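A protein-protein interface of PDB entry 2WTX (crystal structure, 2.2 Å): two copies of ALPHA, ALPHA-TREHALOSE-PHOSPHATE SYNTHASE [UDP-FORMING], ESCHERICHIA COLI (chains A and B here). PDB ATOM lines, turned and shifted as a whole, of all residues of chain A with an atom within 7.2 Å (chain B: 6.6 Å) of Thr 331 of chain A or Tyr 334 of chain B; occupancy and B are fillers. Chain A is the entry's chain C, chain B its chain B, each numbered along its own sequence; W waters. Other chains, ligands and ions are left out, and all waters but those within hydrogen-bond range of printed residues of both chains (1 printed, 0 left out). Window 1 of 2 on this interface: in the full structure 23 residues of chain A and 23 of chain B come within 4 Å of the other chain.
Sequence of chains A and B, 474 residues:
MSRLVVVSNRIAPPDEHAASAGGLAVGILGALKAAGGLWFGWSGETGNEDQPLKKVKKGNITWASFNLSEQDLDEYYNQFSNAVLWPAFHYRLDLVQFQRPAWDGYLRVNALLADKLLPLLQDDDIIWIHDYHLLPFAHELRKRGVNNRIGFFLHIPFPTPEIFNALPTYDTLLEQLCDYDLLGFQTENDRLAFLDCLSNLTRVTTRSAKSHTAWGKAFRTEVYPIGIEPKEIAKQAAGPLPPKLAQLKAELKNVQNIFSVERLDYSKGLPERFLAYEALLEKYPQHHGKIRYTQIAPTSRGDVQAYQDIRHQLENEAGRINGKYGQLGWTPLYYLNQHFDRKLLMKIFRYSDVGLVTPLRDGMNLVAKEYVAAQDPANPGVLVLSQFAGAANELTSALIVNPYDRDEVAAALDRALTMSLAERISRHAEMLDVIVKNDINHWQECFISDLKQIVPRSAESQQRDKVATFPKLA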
ATOM      1  N   TYR A 277     -16.347   1.322 -28.928  1.00  0.00           N
ATOM      2  CA  TYR A 277     -16.266   0.036 -28.244  1.00  0.00           C
ATOM      3  C   TYR A 277     -16.877   0.120 -26.859  1.00  0.00           C
ATOM      4  O   TYR A 277     -17.643  -0.761 -26.480  1.00  0.00           O
ATOM      5  CB  TYR A 277     -14.834  -0.463 -28.136  1.00  0.00           C
ATOM      6  CG  TYR A 277     -14.745  -1.875 -27.593  1.00  0.00           C
ATOM      7  CD1 TYR A 277     -15.465  -2.922 -28.190  1.00  0.00           C
ATOM      8  CD2 TYR A 277     -13.925  -2.177 -26.497  1.00  0.00           C
ATOM      9  CE1 TYR A 277     -15.379  -4.232 -27.697  1.00  0.00           C
ATOM     10  CE2 TYR A 277     -13.830  -3.505 -25.990  1.00  0.00           C
ATOM     11  CZ  TYR A 277     -14.570  -4.525 -26.602  1.00  0.00           C
ATOM     12  OH  TYR A 277     -14.483  -5.840 -26.141  1.00  0.00           O
ATOM     13  N   ILE A 291     -16.855 -11.430 -26.219  1.00  0.00           N
ATOM     14  CA  ILE A 291     -16.187 -10.714 -27.302  1.00  0.00           C
ATOM     15  C   ILE A 291     -14.903 -10.086 -26.782  1.00  0.00           C
ATOM     16  O   ILE A 291     -14.729  -9.917 -25.574  1.00  0.00           O
ATOM     17  CB  ILE A 291     -17.086  -9.606 -27.924  1.00  0.00           C
ATOM     18  CG1 ILE A 291     -17.278  -8.455 -26.927  1.00  0.00           C
ATOM     19  CG2 ILE A 291     -18.417 -10.185 -28.409  1.00  0.00           C
ATOM     20  CD1 ILE A 291     -18.060  -7.289 -27.442  1.00  0.00           C
ATOM     21  N   ARG A 292     -14.017  -9.751 -27.707  1.00  0.00           N
ATOM     22  CA  ARG A 292     -12.758  -9.097 -27.407  1.00  0.00           C
ATOM     23  C   ARG A 292     -12.446  -8.097 -28.524  1.00  0.00           C
ATOM     24  O   ARG A 292     -12.784  -8.335 -29.688  1.00  0.00           O
ATOM     25  CB  ARG A 292     -11.648 -10.134 -27.334  1.00  0.00           C
ATOM     26  CG  ARG A 292     -10.278  -9.546 -27.045  1.00  0.00           C
ATOM     27  CD  ARG A 292      -9.163 -10.572 -27.167  1.00  0.00           C
ATOM     28  NE  ARG A 292      -9.434 -11.763 -26.359  1.00  0.00           N
ATOM     29  CZ  ARG A 292      -8.541 -12.709 -26.073  1.00  0.00           C
ATOM     30  NH1 ARG A 292      -8.910 -13.744 -25.334  1.00  0.00           N
ATOM     31  NH2 ARG A 292      -7.283 -12.620 -26.514  1.00  0.00           N
ATOM     32  N   TYR A 293     -11.817  -6.977 -28.182  1.00  0.00           N
ATOM     33  CA  TYR A 293     -11.317  -6.072 -29.207  1.00  0.00           C
ATOM     34  C   TYR A 293      -9.810  -5.869 -29.068  1.00  0.00           C
ATOM     35  O   TYR A 293      -9.319  -5.456 -28.013  1.00  0.00           O
ATOM     36  CB  TYR A 293     -12.118  -4.767 -29.196  1.00  0.00           C
ATOM     37  CG  TYR A 293     -11.502  -3.558 -29.878  1.00  0.00           C
ATOM     38  CD1 TYR A 293     -11.012  -3.607 -31.192  1.00  0.00           C
ATOM     39  CD2 TYR A 293     -11.483  -2.335 -29.214  1.00  0.00           C
ATOM     40  CE1 TYR A 293     -10.472  -2.459 -31.803  1.00  0.00           C
ATOM     41  CE2 TYR A 293     -10.962  -1.202 -29.802  1.00  0.00           C
ATOM     42  CZ  TYR A 293     -10.453  -1.263 -31.084  1.00  0.00           C
ATOM     43  OH  TYR A 293      -9.935  -0.103 -31.600  1.00  0.00           O
ATOM     44  N   ASN A 322     -10.993  -0.995 -19.639  1.00  0.00           N
ATOM     45  CA  ASN A 322     -10.740  -2.263 -18.967  1.00  0.00           C
ATOM     46  C   ASN A 322     -11.052  -2.245 -17.466  1.00  0.00           C
ATOM     47  O   ASN A 322     -11.513  -3.236 -16.922  1.00  0.00           O
ATOM     48  CB  ASN A 322      -9.306  -2.749 -19.228  1.00  0.00           C
ATOM     49  CG  ASN A 322      -9.139  -3.325 -20.646  1.00  0.00           C
ATOM     50  OD1 ASN A 322     -10.100  -3.837 -21.232  1.00  0.00           O
ATOM     51  ND2 ASN A 322      -7.925  -3.243 -21.195  1.00  0.00           N
ATOM     52  N   GLY A 323     -10.809  -1.114 -16.812  1.00  0.00           N
ATOM     53  CA  GLY A 323     -11.009  -1.011 -15.379  1.00  0.00           C
ATOM     54  C   GLY A 323     -12.487  -1.015 -15.060  1.00  0.00           C
ATOM     55  O   GLY A 323     -12.891  -1.483 -14.009  1.00  0.00           O
ATOM     56  N   TYR A 325     -15.146  -2.303 -17.299  1.00  0.00           N
ATOM     57  CA  TYR A 325     -15.931  -3.403 -17.856  1.00  0.00           C
ATOM     58  C   TYR A 325     -15.258  -4.755 -17.688  1.00  0.00           C
ATOM     59  O   TYR A 325     -15.864  -5.792 -17.976  1.00  0.00           O
ATOM     60  CB  TYR A 325     -16.221  -3.155 -19.335  1.00  0.00           C
ATOM     61  CG  TYR A 325     -17.171  -2.019 -19.553  1.00  0.00           C
ATOM     62  CD1 TYR A 325     -18.543  -2.191 -19.360  1.00  0.00           C
ATOM     63  CD2 TYR A 325     -16.705  -0.752 -19.927  1.00  0.00           C
ATOM     64  CE1 TYR A 325     -19.428  -1.126 -19.545  1.00  0.00           C
ATOM     65  CE2 TYR A 325     -17.575   0.303 -20.114  1.00  0.00           C
ATOM     66  CZ  TYR A 325     -18.932   0.105 -19.936  1.00  0.00           C
ATOM     67  OH  TYR A 325     -19.803   1.154 -20.120  1.00  0.00           O
ATOM     68  N   GLY A 326     -14.003  -4.737 -17.246  1.00  0.00           N
ATOM     69  CA  GLY A 326     -13.228  -5.957 -17.086  1.00  0.00           C
ATOM     70  C   GLY A 326     -13.757  -6.808 -15.952  1.00  0.00           C
ATOM     71  O   GLY A 326     -14.506  -6.329 -15.100  1.00  0.00           O
ATOM     72  N   GLN A 327     -13.351  -8.071 -15.963  1.00  0.00           N
ATOM     73  CA  GLN A 327     -13.732  -9.067 -14.968  1.00  0.00           C
ATOM     74  C   GLN A 327     -12.485  -9.883 -14.662  1.00  0.00           C
ATOM     75  O   GLN A 327     -11.490  -9.813 -15.401  1.00  0.00           O
ATOM     76  CB  GLN A 327     -14.815  -9.997 -15.524  1.00  0.00           C
ATOM     77  CG  GLN A 327     -16.197  -9.382 -15.758  1.00  0.00           C
ATOM     78  CD  GLN A 327     -17.092 -10.257 -16.671  1.00  0.00           C
ATOM     79  OE1 GLN A 327     -16.797 -11.421 -16.921  1.00  0.00           O
ATOM     80  NE2 GLN A 327     -18.165  -9.677 -17.181  1.00  0.00           N
ATOM     81  N   LEU A 328     -12.539 -10.683 -13.592  1.00  0.00           N
ATOM     82  CA  LEU A 328     -11.372 -11.487 -13.189  1.00  0.00           C
ATOM     83  C   LEU A 328     -10.772 -12.334 -14.324  1.00  0.00           C
ATOM     84  O   LEU A 328      -9.545 -12.507 -14.398  1.00  0.00           O
ATOM     85  CB  LEU A 328     -11.682 -12.369 -11.962  1.00  0.00           C
ATOM     86  CG  LEU A 328     -11.922 -11.661 -10.620  1.00  0.00           C
ATOM     87  CD1 LEU A 328     -12.517 -12.628  -9.611  1.00  0.00           C
ATOM     88  CD2 LEU A 328     -10.655 -10.999 -10.056  1.00  0.00           C
ATOM     89  N   GLY A 329     -11.623 -12.853 -15.208  1.00  0.00           N
ATOM     90  CA  GLY A 329     -11.140 -13.686 -16.301  1.00  0.00           C
ATOM     91  C   GLY A 329     -11.479 -13.198 -17.699  1.00  0.00           C
ATOM     92  O   GLY A 329     -11.496 -13.994 -18.654  1.00  0.00           O
ATOM     93  N   TRP A 330     -11.756 -11.901 -17.833  1.00  0.00           N
ATOM     94  CA  TRP A 330     -12.107 -11.317 -19.127  1.00  0.00           C
ATOM     95  C   TRP A 330     -11.684  -9.858 -19.193  1.00  0.00           C
ATOM     96  O   TRP A 330     -12.265  -9.004 -18.509  1.00  0.00           O
ATOM     97  CB  TRP A 330     -13.613 -11.431 -19.395  1.00  0.00           C
ATOM     98  CG  TRP A 330     -14.053 -10.807 -20.712  1.00  0.00           C
ATOM     99  CD1 TRP A 330     -13.686 -11.206 -21.971  1.00  0.00           C
ATOM    100  CD2 TRP A 330     -14.945  -9.684 -20.892  1.00  0.00           C
ATOM    101  NE1 TRP A 330     -14.287 -10.400 -22.918  1.00  0.00           N
ATOM    102  CE2 TRP A 330     -15.069  -9.466 -22.286  1.00  0.00           C
ATOM    103  CE3 TRP A 330     -15.661  -8.857 -20.012  1.00  0.00           C
ATOM    104  CZ2 TRP A 330     -15.874  -8.445 -22.825  1.00  0.00           C
ATOM    105  CZ3 TRP A 330     -16.464  -7.829 -20.549  1.00  0.00           C
ATOM    106  CH2 TRP A 330     -16.564  -7.640 -21.945  1.00  0.00           C
ATOM    107  N   THR A 331     -10.672  -9.605 -20.023  1.00  0.00           N
ATOM    108  CA  THR A 331     -10.178  -8.277 -20.365  1.00  0.00           C
ATOM    109  C   THR A 331     -10.764  -7.864 -21.729  1.00  0.00           C
ATOM    110  O   THR A 331     -10.400  -8.439 -22.754  1.00  0.00           O
ATOM    111  CB  THR A 331      -8.638  -8.296 -20.418  1.00  0.00           C
ATOM    112  OG1 THR A 331      -8.123  -8.397 -19.085  1.00  0.00           O
ATOM    113  CG2 THR A 331      -8.068  -7.032 -21.063  1.00  0.00           C
ATOM    114  N   PRO A 332     -11.684  -6.875 -21.737  1.00  0.00           N
ATOM    115  CA  PRO A 332     -12.448  -6.513 -22.932  1.00  0.00           C
ATOM    116  C   PRO A 332     -11.615  -5.956 -24.082  1.00  0.00           C
ATOM    117  O   PRO A 332     -11.982  -6.147 -25.252  1.00  0.00           O
ATOM    118  CB  PRO A 332     -13.410  -5.428 -22.429  1.00  0.00           C
ATOM    119  CG  PRO A 332     -13.431  -5.573 -20.957  1.00  0.00           C
ATOM    120  CD  PRO A 332     -12.078  -6.059 -20.580  1.00  0.00           C
ATOM    121  N   LEU A 333     -10.513  -5.291 -23.743  1.00  0.00           N
ATOM    122  CA  LEU A 333      -9.736  -4.511 -24.703  1.00  0.00           C
ATOM    123  C   LEU A 333      -8.249  -4.841 -24.630  1.00  0.00           C
ATOM    124  O   LEU A 333      -7.627  -4.713 -23.573  1.00  0.00           O
ATOM    125  CB  LEU A 333      -9.961  -3.012 -24.440  1.00  0.00           C
ATOM    126  CG  LEU A 333      -9.637  -1.978 -25.523  1.00  0.00           C
ATOM    127  CD1 LEU A 333     -10.154  -0.608 -25.106  1.00  0.00           C
ATOM    128  CD2 LEU A 333      -8.145  -1.904 -25.827  1.00  0.00           C
ATOM    129  N   TYR A 334      -7.681  -5.264 -25.752  1.00  0.00           N
ATOM    130  CA  TYR A 334      -6.242  -5.510 -25.850  1.00  0.00           C
ATOM    131  C   TYR A 334      -5.647  -4.415 -26.733  1.00  0.00           C
ATOM    132  O   TYR A 334      -5.844  -4.417 -27.947  1.00  0.00           O
ATOM    133  CB  TYR A 334      -5.950  -6.876 -26.477  1.00  0.00           C
ATOM    134  CG  TYR A 334      -6.126  -8.093 -25.589  1.00  0.00           C
ATOM    135  CD1 TYR A 334      -7.220  -8.219 -24.726  1.00  0.00           C
ATOM    136  CD2 TYR A 334      -5.220  -9.155 -25.659  1.00  0.00           C
ATOM    137  CE1 TYR A 334      -7.387  -9.358 -23.917  1.00  0.00           C
ATOM    138  CE2 TYR A 334      -5.376 -10.293 -24.869  1.00  0.00           C
ATOM    139  CZ  TYR A 334      -6.460 -10.387 -23.995  1.00  0.00           C
ATOM    140  OH  TYR A 334      -6.620 -11.517 -23.212  1.00  0.00           O
ATOM    141  N   TYR A 335      -4.929  -3.482 -26.125  1.00  0.00           N
ATOM    142  CA  TYR A 335      -4.256  -2.433 -26.863  1.00  0.00           C
ATOM    143  C   TYR A 335      -2.767  -2.700 -26.850  1.00  0.00           C
ATOM    144  O   TYR A 335      -2.179  -2.853 -25.794  1.00  0.00           O
ATOM    145  CB  TYR A 335      -4.581  -1.056 -26.256  1.00  0.00           C
ATOM    146  CG  TYR A 335      -3.594   0.018 -26.615  1.00  0.00           C
ATOM    147  CD1 TYR A 335      -3.491   0.498 -27.928  1.00  0.00           C
ATOM    148  CD2 TYR A 335      -2.728   0.536 -25.651  1.00  0.00           C
ATOM    149  CE1 TYR A 335      -2.559   1.504 -28.262  1.00  0.00           C
ATOM    150  CE2 TYR A 335      -1.789   1.529 -25.972  1.00  0.00           C
ATOM    151  CZ  TYR A 335      -1.716   2.008 -27.274  1.00  0.00           C
ATOM    152  OH  TYR A 335      -0.790   2.987 -27.573  1.00  0.00           O
ATOM    153  N   PHE B 274       2.987  -0.738  -9.965  1.00  0.00           N
ATOM    154  CA  PHE B 274       2.940  -0.989 -11.392  1.00  0.00           C
ATOM    155  C   PHE B 274       4.334  -0.896 -12.016  1.00  0.00           C
ATOM    156  O   PHE B 274       4.676  -1.707 -12.881  1.00  0.00           O
ATOM    157  CB  PHE B 274       1.972  -0.017 -12.078  1.00  0.00           C
ATOM    158  CG  PHE B 274       0.514  -0.406 -11.958  1.00  0.00           C
ATOM    159  CD1 PHE B 274       0.051  -1.165 -10.887  1.00  0.00           C
ATOM    160  CD2 PHE B 274      -0.408   0.038 -12.894  1.00  0.00           C
ATOM    161  CE1 PHE B 274      -1.294  -1.508 -10.768  1.00  0.00           C
ATOM    162  CE2 PHE B 274      -1.749  -0.298 -12.783  1.00  0.00           C
ATOM    163  CZ  PHE B 274      -2.191  -1.083 -11.713  1.00  0.00           C
ATOM    164  N   TYR B 277       6.259  -4.000 -11.250  1.00  0.00           N
ATOM    165  CA  TYR B 277       5.847  -5.111 -12.096  1.00  0.00           C
ATOM    166  C   TYR B 277       6.429  -4.957 -13.481  1.00  0.00           C
ATOM    167  O   TYR B 277       6.806  -5.944 -14.113  1.00  0.00           O
ATOM    168  CB  TYR B 277       4.320  -5.201 -12.187  1.00  0.00           C
ATOM    169  CG  TYR B 277       3.787  -6.389 -12.979  1.00  0.00           C
ATOM    170  CD1 TYR B 277       4.038  -7.687 -12.569  1.00  0.00           C
ATOM    171  CD2 TYR B 277       2.997  -6.206 -14.090  1.00  0.00           C
ATOM    172  CE1 TYR B 277       3.551  -8.776 -13.263  1.00  0.00           C
ATOM    173  CE2 TYR B 277       2.484  -7.297 -14.796  1.00  0.00           C
ATOM    174  CZ  TYR B 277       2.775  -8.581 -14.369  1.00  0.00           C
ATOM    175  OH  TYR B 277       2.276  -9.670 -15.031  1.00  0.00           O
ATOM    176  N   ARG B 292       0.517 -13.393 -14.195  1.00  0.00           N
ATOM    177  CA  ARG B 292      -0.480 -12.351 -14.310  1.00  0.00           C
ATOM    178  C   ARG B 292      -0.517 -11.613 -12.971  1.00  0.00           C
ATOM    179  O   ARG B 292      -0.426 -12.224 -11.906  1.00  0.00           O
ATOM    180  CB  ARG B 292      -1.848 -12.958 -14.587  1.00  0.00           C
ATOM    181  CG  ARG B 292      -2.973 -11.948 -14.658  1.00  0.00           C
ATOM    182  CD  ARG B 292      -4.320 -12.651 -14.753  1.00  0.00           C
ATOM    183  NE  ARG B 292      -4.362 -13.542 -15.905  1.00  0.00           N
ATOM    184  CZ  ARG B 292      -5.413 -14.273 -16.258  1.00  0.00           C
ATOM    185  NH1 ARG B 292      -5.338 -15.042 -17.331  1.00  0.00           N
ATOM    186  NH2 ARG B 292      -6.538 -14.240 -15.543  1.00  0.00           N
ATOM    187  N   TYR B 293      -0.637 -10.297 -13.043  1.00  0.00           N
ATOM    188  CA  TYR B 293      -0.810  -9.472 -11.869  1.00  0.00           C
ATOM    189  C   TYR B 293      -2.210  -8.890 -11.973  1.00  0.00           C
ATOM    190  O   TYR B 293      -2.542  -8.261 -12.960  1.00  0.00           O
ATOM    191  CB  TYR B 293       0.297  -8.406 -11.850  1.00  0.00           C
ATOM    192  CG  TYR B 293       0.097  -7.204 -10.946  1.00  0.00           C
ATOM    193  CD1 TYR B 293      -0.540  -7.318  -9.706  1.00  0.00           C
ATOM    194  CD2 TYR B 293       0.570  -5.955 -11.330  1.00  0.00           C
ATOM    195  CE1 TYR B 293      -0.723  -6.208  -8.883  1.00  0.00           C
ATOM    196  CE2 TYR B 293       0.395  -4.831 -10.508  1.00  0.00           C
ATOM    197  CZ  TYR B 293      -0.259  -4.976  -9.290  1.00  0.00           C
ATOM    198  OH  TYR B 293      -0.440  -3.892  -8.480  1.00  0.00           O
ATOM    199  N   THR B 294      -3.049  -9.147 -10.980  1.00  0.00           N
ATOM    200  CA  THR B 294      -4.383  -8.551 -10.948  1.00  0.00           C
ATOM    201  C   THR B 294      -4.449  -7.524  -9.812  1.00  0.00           C
ATOM    202  O   THR B 294      -4.124  -7.836  -8.665  1.00  0.00           O
ATOM    203  CB  THR B 294      -5.478  -9.644 -10.803  1.00  0.00           C
ATOM    204  OG1 THR B 294      -5.300 -10.628 -11.828  1.00  0.00           O
ATOM    205  CG2 THR B 294      -6.880  -9.061 -10.938  1.00  0.00           C
ATOM    206  N   GLN B 295      -4.838  -6.298 -10.154  1.00  0.00           N
ATOM    207  CA  GLN B 295      -4.996  -5.231  -9.183  1.00  0.00           C
ATOM    208  C   GLN B 295      -6.458  -4.861  -9.097  1.00  0.00           C
ATOM    209  O   GLN B 295      -7.082  -4.422 -10.078  1.00  0.00           O
ATOM    210  CB  GLN B 295      -4.170  -3.991  -9.569  1.00  0.00           C
ATOM    211  CG  GLN B 295      -4.377  -2.803  -8.644  1.00  0.00           C
ATOM    212  CD  GLN B 295      -3.762  -3.028  -7.265  1.00  0.00           C
ATOM    213  OE1 GLN B 295      -2.562  -3.261  -7.154  1.00  0.00           O
ATOM    214  NE2 GLN B 295      -4.591  -2.969  -6.205  1.00  0.00           N
ATOM    215  N   ILE B 296      -7.012  -5.051  -7.920  1.00  0.00           N
ATOM    216  CA  ILE B 296      -8.364  -4.612  -7.679  1.00  0.00           C
ATOM    217  C   ILE B 296      -8.286  -3.301  -6.923  1.00  0.00           C
ATOM    218  O   ILE B 296      -7.674  -3.240  -5.874  1.00  0.00           O
ATOM    219  CB  ILE B 296      -9.143  -5.685  -6.925  1.00  0.00           C
ATOM    220  CG1 ILE B 296      -9.259  -6.922  -7.839  1.00  0.00           C
ATOM    221  CG2 ILE B 296     -10.508  -5.145  -6.489  1.00  0.00           C
ATOM    222  CD1 ILE B 296     -10.182  -7.984  -7.333  1.00  0.00           C
ATOM    223  N   ALA B 318      -1.511   1.403 -16.515  1.00  0.00           N
ATOM    224  CA  ALA B 318      -2.095   0.124 -16.969  1.00  0.00           C
ATOM    225  C   ALA B 318      -2.092   0.022 -18.495  1.00  0.00           C
ATOM    226  O   ALA B 318      -1.710  -1.005 -19.051  1.00  0.00           O
ATOM    227  CB  ALA B 318      -3.535  -0.073 -16.417  1.00  0.00           C
ATOM    228  N   ASN B 322       0.619  -2.664 -20.415  1.00  0.00           N
ATOM    229  CA  ASN B 322       0.001  -3.663 -21.295  1.00  0.00           C
ATOM    230  C   ASN B 322       0.268  -3.414 -22.784  1.00  0.00           C
ATOM    231  O   ASN B 322       0.437  -4.363 -23.548  1.00  0.00           O
ATOM    232  CB  ASN B 322      -1.509  -3.778 -21.049  1.00  0.00           C
ATOM    233  CG  ASN B 322      -1.840  -4.557 -19.778  1.00  0.00           C
ATOM    234  OD1 ASN B 322      -1.092  -5.450 -19.337  1.00  0.00           O
ATOM    235  ND2 ASN B 322      -2.964  -4.217 -19.180  1.00  0.00           N
ATOM    236  N   TRP B 330      -1.689 -12.941 -24.468  1.00  0.00           N
ATOM    237  CA  TRP B 330      -1.268 -12.700 -23.075  1.00  0.00           C
ATOM    238  C   TRP B 330      -1.223 -11.228 -22.670  1.00  0.00           C
ATOM    239  O   TRP B 330      -0.399 -10.452 -23.175  1.00  0.00           O
ATOM    240  CB  TRP B 330       0.102 -13.311 -22.817  1.00  0.00           C
ATOM    241  CG  TRP B 330       0.583 -13.149 -21.384  1.00  0.00           C
ATOM    242  CD1 TRP B 330      -0.004 -13.661 -20.259  1.00  0.00           C
ATOM    243  CD2 TRP B 330       1.769 -12.476 -20.944  1.00  0.00           C
ATOM    244  NE1 TRP B 330       0.732 -13.337 -19.147  1.00  0.00           N
ATOM    245  CE2 TRP B 330       1.827 -12.612 -19.535  1.00  0.00           C
ATOM    246  CE3 TRP B 330       2.783 -11.761 -21.599  1.00  0.00           C
ATOM    247  CZ2 TRP B 330       2.861 -12.053 -18.763  1.00  0.00           C
ATOM    248  CZ3 TRP B 330       3.820 -11.214 -20.826  1.00  0.00           C
ATOM    249  CH2 TRP B 330       3.845 -11.365 -19.426  1.00  0.00           C
ATOM    250  N   THR B 331      -2.111 -10.867 -21.744  1.00  0.00           N
ATOM    251  CA  THR B 331      -2.121  -9.556 -21.109  1.00  0.00           C
ATOM    252  C   THR B 331      -1.462  -9.611 -19.715  1.00  0.00           C
ATOM    253  O   THR B 331      -1.980 -10.269 -18.813  1.00  0.00           O
ATOM    254  CB  THR B 331      -3.557  -9.049 -21.016  1.00  0.00           C
ATOM    255  OG1 THR B 331      -4.098  -8.990 -22.345  1.00  0.00           O
ATOM    256  CG2 THR B 331      -3.615  -7.665 -20.389  1.00  0.00           C
ATOM    257  N   PRO B 332      -0.317  -8.920 -19.534  1.00  0.00           N
ATOM    258  CA  PRO B 332       0.412  -9.021 -18.255  1.00  0.00           C
ATOM    259  C   PRO B 332      -0.340  -8.477 -17.027  1.00  0.00           C
ATOM    260  O   PRO B 332      -0.158  -9.002 -15.928  1.00  0.00           O
ATOM    261  CB  PRO B 332       1.697  -8.224 -18.490  1.00  0.00           C
ATOM    262  CG  PRO B 332       1.754  -7.928 -19.944  1.00  0.00           C
ATOM    263  CD  PRO B 332       0.399  -8.112 -20.536  1.00  0.00           C
ATOM    264  N   LEU B 333      -1.190  -7.471 -17.212  1.00  0.00           N
ATOM    265  CA  LEU B 333      -1.758  -6.750 -16.071  1.00  0.00           C
ATOM    266  C   LEU B 333      -3.269  -6.538 -16.196  1.00  0.00           C
ATOM    267  O   LEU B 333      -3.757  -6.031 -17.217  1.00  0.00           O
ATOM    268  CB  LEU B 333      -1.014  -5.416 -15.879  1.00  0.00           C
ATOM    269  CG  LEU B 333      -1.220  -4.569 -14.623  1.00  0.00           C
ATOM    270  CD1 LEU B 333      -0.075  -3.552 -14.467  1.00  0.00           C
ATOM    271  CD2 LEU B 333      -2.565  -3.852 -14.661  1.00  0.00           C
ATOM    272  N   TYR B 334      -4.000  -6.935 -15.155  1.00  0.00           N
ATOM    273  CA  TYR B 334      -5.452  -6.802 -15.143  1.00  0.00           C
ATOM    274  C   TYR B 334      -5.821  -5.776 -14.071  1.00  0.00           C
ATOM    275  O   TYR B 334      -5.680  -6.036 -12.877  1.00  0.00           O
ATOM    276  CB  TYR B 334      -6.148  -8.151 -14.879  1.00  0.00           C
ATOM    277  CG  TYR B 334      -6.111  -9.173 -16.025  1.00  0.00           C
ATOM    278  CD1 TYR B 334      -4.928  -9.483 -16.681  1.00  0.00           C
ATOM    279  CD2 TYR B 334      -7.259  -9.871 -16.399  1.00  0.00           C
ATOM    280  CE1 TYR B 334      -4.891 -10.419 -17.725  1.00  0.00           C
ATOM    281  CE2 TYR B 334      -7.234 -10.821 -17.440  1.00  0.00           C
ATOM    282  CZ  TYR B 334      -6.043 -11.079 -18.099  1.00  0.00           C
ATOM    283  OH  TYR B 334      -5.989 -12.007 -19.118  1.00  0.00           O
ATOM    284  N   TYR B 335      -6.273  -4.606 -14.502  1.00  0.00           N
ATOM    285  CA  TYR B 335      -6.649  -3.555 -13.584  1.00  0.00           C
ATOM    286  C   TYR B 335      -8.181  -3.470 -13.476  1.00  0.00           C
ATOM    287  O   TYR B 335      -8.876  -3.270 -14.468  1.00  0.00           O
ATOM    288  CB  TYR B 335      -5.994  -2.237 -14.010  1.00  0.00           C
ATOM    289  CG  TYR B 335      -6.649  -0.995 -13.463  1.00  0.00           C
ATOM    290  CD1 TYR B 335      -6.559  -0.650 -12.102  1.00  0.00           C
ATOM    291  CD2 TYR B 335      -7.354  -0.152 -14.318  1.00  0.00           C
ATOM    292  CE1 TYR B 335      -7.185   0.521 -11.623  1.00  0.00           C
ATOM    293  CE2 TYR B 335      -7.963   0.996 -13.864  1.00  0.00           C
ATOM    294  CZ  TYR B 335      -7.889   1.329 -12.517  1.00  0.00           C
ATOM    295  OH  TYR B 335      -8.530   2.480 -12.119  1.00  0.00           O
ATOM    296  N   LEU B 336      -8.699  -3.663 -12.269  1.00  0.00           N
ATOM    297  CA  LEU B 336     -10.149  -3.639 -12.057  1.00  0.00           C
ATOM    298  C   LEU B 336     -10.526  -2.567 -11.048  1.00  0.00           C
ATOM    299  O   LEU B 336     -10.265  -2.713  -9.850  1.00  0.00           O
ATOM    300  CB  LEU B 336     -10.677  -5.023 -11.625  1.00  0.00           C
ATOM    301  CG  LEU B 336     -10.298  -6.213 -12.522  1.00  0.00           C
ATOM    302  CD1 LEU B 336     -10.706  -7.561 -11.900  1.00  0.00           C
ATOM    303  CD2 LEU B 336     -10.933  -6.050 -13.887  1.00  0.00           C
HETATM  304  O   HOH W   1      -7.374 -12.082 -12.817  1.00  0.00           O
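The side-chain amide nitrogen (ND2) of Asn 322 of chain B lies close to the backbone carbonyl oxygen (O) of Ala 318 of chain B, 3.5 Å away.
O of Gln 295 of chain B sits at hydrogen-bond distance from N of Leu 336 of chain B, at 2.8 Å.
The backbone carbonyl oxygen (O) of Leu 333 of chain B sits at hydrogen-bond distance from the side-chain amide nitrogen (ND2) of Asn 322 of chain B (2.8 Å).
The backbone NH (N) of Gln 295 of chain B lies within hydrogen-bond range of the backbone carbonyl oxygen (O) of Tyr 334 of chain B (2.9 Å).
Of the 16 printed residues of chain B, 6 touch a printed residue of chain A.
Printed residues of chain B that touch a printed residue of chain A: Arg 292, Asn 322, Thr 331, Tyr 334, Tyr 335 and Leu 336.
Hydrophobic or aromatic side chains of chain B that line the printed part of chain A: Tyr 334, Tyr 335 and Leu 336.
Along chain B the printed residues that touch a printed residue of chain A span positions 292 to 336.
Along chain A the printed residues that touch a printed residue of chain B span positions 322 to 335.
Asn 322 of chain A touches Tyr 335 of chain B (O to O, 3.6 Å).
Tyr 335 of chain B touches Gly 323 of chain A (O to CA, 3.2 Å).
Gly 326 of chain A touches Leu 336 of chain B (C to CD2, 3.6 Å).
Leu 336 of chain B touches Gln 327 of chain A (CD2 to N, 3.8 Å).
Leu 328 of chain A touches Leu 336 of chain B.
Thr 331 of chain A touches Tyr 334 of chain B (OG1 to CE2, 3.1 Å).
OG1 of Thr 331 of chain B touches CE2 of Tyr 334 of chain A (3.1 Å).
O of Tyr 335 of chain A touches O of Asn 322 of chain B, 3.8 Å away.
Thr 331 of chain A touches just one residue of chain B: Tyr 334 (3.1 Å).
Tyr 334 of chain B touches just one residue of chain A: Thr 331.
Printed residues of chain B within 4 Å of Asn 322 of chain A: Tyr 335.
Printed residues of chain B within 4 Å of Tyr 335 of chain A: Asn 322.
Ile 291 of chain A touches none of the printed residues of chain B.
The nearest residue of chain A that does not touch Tyr 334 of chain B is Leu 328 of chain A (4.02 Å).
Asn 322 of chain A touches Tyr 335 of chain B, and with the chains exchanged Tyr 335 of chain A touches Asn 322 of chain B.
Thr 331 of chain A touches Tyr 334 of chain B, and with the chains exchanged Tyr 334 of chain A touches Thr 331 of chain B.
Positions printed for both chains: 277, 292, 293, 322, 330, 331, 332, 333, 334 and 335.
Water W1 lies within hydrogen-bond range of O of Leu 328 of chain A and OG1 of Thr 294 of chain B.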
